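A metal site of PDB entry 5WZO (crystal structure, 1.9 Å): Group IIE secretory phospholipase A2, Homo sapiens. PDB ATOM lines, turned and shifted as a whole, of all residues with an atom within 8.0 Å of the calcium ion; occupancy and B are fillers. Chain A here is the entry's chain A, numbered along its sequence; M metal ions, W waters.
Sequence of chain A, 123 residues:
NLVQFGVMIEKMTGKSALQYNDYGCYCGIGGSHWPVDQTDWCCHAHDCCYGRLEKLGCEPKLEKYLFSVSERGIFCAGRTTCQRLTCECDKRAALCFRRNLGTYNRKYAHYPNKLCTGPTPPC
The backbone carbonyl oxygen (O) of Tyr 26 binds the calcium ion, 2.3 Å away. The calcium ion is bound by the backbone carbonyl oxygen (O) of Gly 28 (2.3 Å). O of Gly 30 is bound to the calcium ion (2.4 Å). The calcium ion is bound by the side-chain carboxylate (OD2) of Asp 47 (2.5 Å). The side-chain carboxylate (OD1) of Asp 47 is bound to the calcium ion (2.5 Å). The calcium ion is bound by water W2 (2.6 Å). The calcium ion is bound by water W1 (2.6 Å).
The backbone NH of Tyr 26 is in hydrogen-bond range of the side-chain carboxylate of Asp 40, at 2.8 Å. The side-chain hydroxyl (OH) of Tyr 26 lies close to the backbone carbonyl oxygen (O) of Ser 32 (3.5 Å). The backbone carbonyl oxygen (O) of Asn 21 sits close to the backbone NH (N) of Gly 28 (3.4 Å). SG of Cys 27 forms a disulfide with SG of Cys 43 (2.0 Å).
Along chain A the residues within 4 Å of the calcium ion span positions 26 to 47. The nearest printed residue that does not touch the calcium ion is Ile 29 (4.1 Å).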
ATOM      1  N   ASN A  21      30.613  -9.625  -6.959  1.00  0.00           N
ATOM      2  CA  ASN A  21      30.812  -9.607  -8.392  1.00  0.00           C
ATOM      3  C   ASN A  21      31.706 -10.751  -8.869  1.00  0.00           C
ATOM      4  O   ASN A  21      31.933 -10.870 -10.078  1.00  0.00           O
ATOM      5  CB  ASN A  21      31.270  -8.236  -8.927  1.00  0.00           C
ATOM      6  CG  ASN A  21      32.660  -7.836  -8.449  1.00  0.00           C
ATOM      7  OD1 ASN A  21      33.263  -8.489  -7.563  1.00  0.00           O
ATOM      8  ND2 ASN A  21      33.188  -6.758  -9.030  1.00  0.00           N
ATOM      9  N   TYR A  23      31.514 -14.265  -7.125  1.00  0.00           N
ATOM     10  CA  TYR A  23      31.116 -15.287  -6.163  1.00  0.00           C
ATOM     11  C   TYR A  23      30.569 -16.517  -6.847  1.00  0.00           C
ATOM     12  O   TYR A  23      29.847 -16.389  -7.834  1.00  0.00           O
ATOM     13  CB  TYR A  23      30.050 -14.678  -5.293  1.00  0.00           C
ATOM     14  CG  TYR A  23      29.495 -15.512  -4.135  1.00  0.00           C
ATOM     15  CD1 TYR A  23      28.477 -16.468  -4.342  1.00  0.00           C
ATOM     16  CD2 TYR A  23      29.937 -15.268  -2.828  1.00  0.00           C
ATOM     17  CE1 TYR A  23      27.942 -17.181  -3.288  1.00  0.00           C
ATOM     18  CE2 TYR A  23      29.419 -15.987  -1.760  1.00  0.00           C
ATOM     19  CZ  TYR A  23      28.407 -16.932  -1.986  1.00  0.00           C
ATOM     20  OH  TYR A  23      27.856 -17.623  -0.903  1.00  0.00           O
ATOM     21  N   CYS A  25      29.780 -19.817  -9.073  1.00  0.00           N
ATOM     22  CA  CYS A  25      29.954 -20.175 -10.462  1.00  0.00           C
ATOM     23  C   CYS A  25      29.276 -19.186 -11.404  1.00  0.00           C
ATOM     24  O   CYS A  25      29.581 -19.198 -12.596  1.00  0.00           O
ATOM     25  CB  CYS A  25      29.462 -21.614 -10.694  1.00  0.00           C
ATOM     26  SG  CYS A  25      30.524 -22.768  -9.747  1.00  0.00           S
ATOM     27  N   TYR A  26      28.366 -18.352 -10.873  1.00  0.00           N
ATOM     28  CA  TYR A  26      27.569 -17.417 -11.705  1.00  0.00           C
ATOM     29  C   TYR A  26      27.747 -15.918 -11.458  1.00  0.00           C
ATOM     30  O   TYR A  26      27.449 -15.117 -12.354  1.00  0.00           O
ATOM     31  CB  TYR A  26      26.066 -17.788 -11.644  1.00  0.00           C
ATOM     32  CG  TYR A  26      25.803 -19.018 -12.445  1.00  0.00           C
ATOM     33  CD1 TYR A  26      25.994 -20.285 -11.888  1.00  0.00           C
ATOM     34  CD2 TYR A  26      25.472 -18.930 -13.825  1.00  0.00           C
ATOM     35  CE1 TYR A  26      25.848 -21.439 -12.654  1.00  0.00           C
ATOM     36  CE2 TYR A  26      25.319 -20.076 -14.600  1.00  0.00           C
ATOM     37  CZ  TYR A  26      25.526 -21.324 -14.009  1.00  0.00           C
ATOM     38  OH  TYR A  26      25.345 -22.486 -14.720  1.00  0.00           O
ATOM     39  N   CYS A  27      28.187 -15.520 -10.265  1.00  0.00           N
ATOM     40  CA  CYS A  27      28.284 -14.073  -9.970  1.00  0.00           C
ATOM     41  C   CYS A  27      29.584 -13.567 -10.578  1.00  0.00           C
ATOM     42  O   CYS A  27      30.654 -13.964 -10.166  1.00  0.00           O
ATOM     43  CB  CYS A  27      28.230 -13.779  -8.483  1.00  0.00           C
ATOM     44  SG  CYS A  27      26.850 -14.493  -7.563  1.00  0.00           S
ATOM     45  N   GLY A  28      29.479 -12.659 -11.542  1.00  0.00           N
ATOM     46  CA  GLY A  28      30.668 -12.355 -12.361  1.00  0.00           C
ATOM     47  C   GLY A  28      30.447 -12.710 -13.805  1.00  0.00           C
ATOM     48  O   GLY A  28      29.354 -13.155 -14.169  1.00  0.00           O
ATOM     49  N   ILE A  29      31.444 -12.527 -14.654  1.00  0.00           N
ATOM     50  CA  ILE A  29      31.156 -12.640 -16.094  1.00  0.00           C
ATOM     51  C   ILE A  29      30.905 -14.087 -16.540  1.00  0.00           C
ATOM     52  O   ILE A  29      31.612 -15.022 -16.122  1.00  0.00           O
ATOM     53  CB  ILE A  29      32.158 -11.838 -16.986  1.00  0.00           C
ATOM     54  CG1 ILE A  29      33.550 -12.461 -16.978  1.00  0.00           C
ATOM     55  CG2 ILE A  29      32.195 -10.353 -16.590  1.00  0.00           C
ATOM     56  CD1 ILE A  29      33.824 -13.326 -18.198  1.00  0.00           C
ATOM     57  N   GLY A  30      29.865 -14.291 -17.336  1.00  0.00           N
ATOM     58  CA  GLY A  30      29.434 -15.647 -17.703  1.00  0.00           C
ATOM     59  C   GLY A  30      28.999 -16.491 -16.512  1.00  0.00           C
ATOM     60  O   GLY A  30      28.524 -15.984 -15.505  1.00  0.00           O
ATOM     61  N   GLY A  31      29.180 -17.796 -16.611  1.00  0.00           N
ATOM     62  CA  GLY A  31      28.591 -18.706 -15.672  1.00  0.00           C
ATOM     63  C   GLY A  31      28.354 -20.016 -16.386  1.00  0.00           C
ATOM     64  O   GLY A  31      28.011 -20.030 -17.536  1.00  0.00           O
ATOM     65  N   SER A  32      28.555 -21.115 -15.678  1.00  0.00           N
ATOM     66  CA  SER A  32      28.391 -22.480 -16.217  1.00  0.00           C
ATOM     67  C   SER A  32      28.324 -23.430 -15.006  1.00  0.00           C
ATOM     68  O   SER A  32      28.667 -23.050 -13.865  1.00  0.00           O
ATOM     69  CB  SER A  32      29.620 -22.839 -17.031  1.00  0.00           C
ATOM     70  OG  SER A  32      30.776 -22.705 -16.202  1.00  0.00           O
ATOM     71  N   ASP A  40      24.458 -17.859  -5.312  1.00  0.00           N
ATOM     72  CA  ASP A  40      24.845 -18.176  -6.696  1.00  0.00           C
ATOM     73  C   ASP A  40      23.632 -18.311  -7.596  1.00  0.00           C
ATOM     74  O   ASP A  40      23.684 -17.884  -8.745  1.00  0.00           O
ATOM     75  CB  ASP A  40      25.714 -19.455  -6.736  1.00  0.00           C
ATOM     76  CG  ASP A  40      26.745 -19.448  -7.830  1.00  0.00           C
ATOM     77  OD1 ASP A  40      26.954 -18.374  -8.460  1.00  0.00           O
ATOM     78  OD2 ASP A  40      27.418 -20.527  -8.056  1.00  0.00           O
ATOM     79  N   CYS A  43      22.505 -15.230  -8.957  1.00  0.00           N
ATOM     80  CA  CYS A  43      23.297 -14.780 -10.113  1.00  0.00           C
ATOM     81  C   CYS A  43      22.992 -15.568 -11.394  1.00  0.00           C
ATOM     82  O   CYS A  43      23.001 -14.982 -12.494  1.00  0.00           O
ATOM     83  CB  CYS A  43      24.801 -14.868  -9.825  1.00  0.00           C
ATOM     84  SG  CYS A  43      25.263 -13.693  -8.538  1.00  0.00           S
ATOM     85  N   HIS A  44      22.762 -16.886 -11.261  1.00  0.00           N
ATOM     86  CA  HIS A  44      22.223 -17.670 -12.388  1.00  0.00           C
ATOM     87  C   HIS A  44      20.939 -17.000 -12.968  1.00  0.00           C
ATOM     88  O   HIS A  44      20.832 -16.755 -14.179  1.00  0.00           O
ATOM     89  CB  HIS A  44      21.921 -19.107 -11.936  1.00  0.00           C
ATOM     90  CG  HIS A  44      21.335 -19.963 -13.037  1.00  0.00           C
ATOM     91  ND1 HIS A  44      19.975 -20.027 -13.285  1.00  0.00           N
ATOM     92  CD2 HIS A  44      21.935 -20.752 -13.947  1.00  0.00           C
ATOM     93  CE1 HIS A  44      19.766 -20.842 -14.304  1.00  0.00           C
ATOM     94  NE2 HIS A  44      20.939 -21.315 -14.713  1.00  0.00           N
ATOM     95  N   HIS A  46      19.873 -13.827 -12.551  1.00  0.00           N
ATOM     96  CA  HIS A  46      20.248 -12.495 -13.036  1.00  0.00           C
ATOM     97  C   HIS A  46      20.872 -12.567 -14.429  1.00  0.00           C
ATOM     98  O   HIS A  46      20.538 -11.788 -15.314  1.00  0.00           O
ATOM     99  CB  HIS A  46      21.249 -11.867 -12.056  1.00  0.00           C
ATOM    100  CG  HIS A  46      21.568 -10.436 -12.346  1.00  0.00           C
ATOM    101  ND1 HIS A  46      22.796 -10.034 -12.836  1.00  0.00           N
ATOM    102  CD2 HIS A  46      20.818  -9.319 -12.230  1.00  0.00           C
ATOM    103  CE1 HIS A  46      22.782  -8.717 -12.993  1.00  0.00           C
ATOM    104  NE2 HIS A  46      21.603  -8.263 -12.615  1.00  0.00           N
ATOM    105  N   ASP A  47      21.782 -13.523 -14.628  1.00  0.00           N
ATOM    106  CA  ASP A  47      22.329 -13.774 -15.946  1.00  0.00           C
ATOM    107  C   ASP A  47      21.205 -14.055 -16.975  1.00  0.00           C
ATOM    108  O   ASP A  47      21.261 -13.556 -18.106  1.00  0.00           O
ATOM    109  CB  ASP A  47      23.233 -15.000 -15.857  1.00  0.00           C
ATOM    110  CG  ASP A  47      24.620 -14.693 -15.299  1.00  0.00           C
ATOM    111  OD1 ASP A  47      24.890 -13.540 -14.858  1.00  0.00           O
ATOM    112  OD2 ASP A  47      25.460 -15.623 -15.326  1.00  0.00           O
ATOM    113  N   CYS A  48      20.225 -14.887 -16.590  1.00  0.00           N
ATOM    114  CA  CYS A  48      19.083 -15.219 -17.442  1.00  0.00           C
ATOM    115  C   CYS A  48      18.270 -13.970 -17.715  1.00  0.00           C
ATOM    116  O   CYS A  48      17.761 -13.767 -18.830  1.00  0.00           O
ATOM    117  CB  CYS A  48      18.153 -16.229 -16.724  1.00  0.00           C
ATOM    118  SG  CYS A  48      18.914 -17.861 -16.593  1.00  0.00           S
HETATM  119 CA    CA M   1      27.307 -14.233 -14.483  1.00  0.00          CA
HETATM  120  O   HOH W   1      27.113 -11.988 -13.131  1.00  0.00           O
HETATM  121  O   HOH W   2      27.148 -12.952 -16.763  1.00  0.00           O
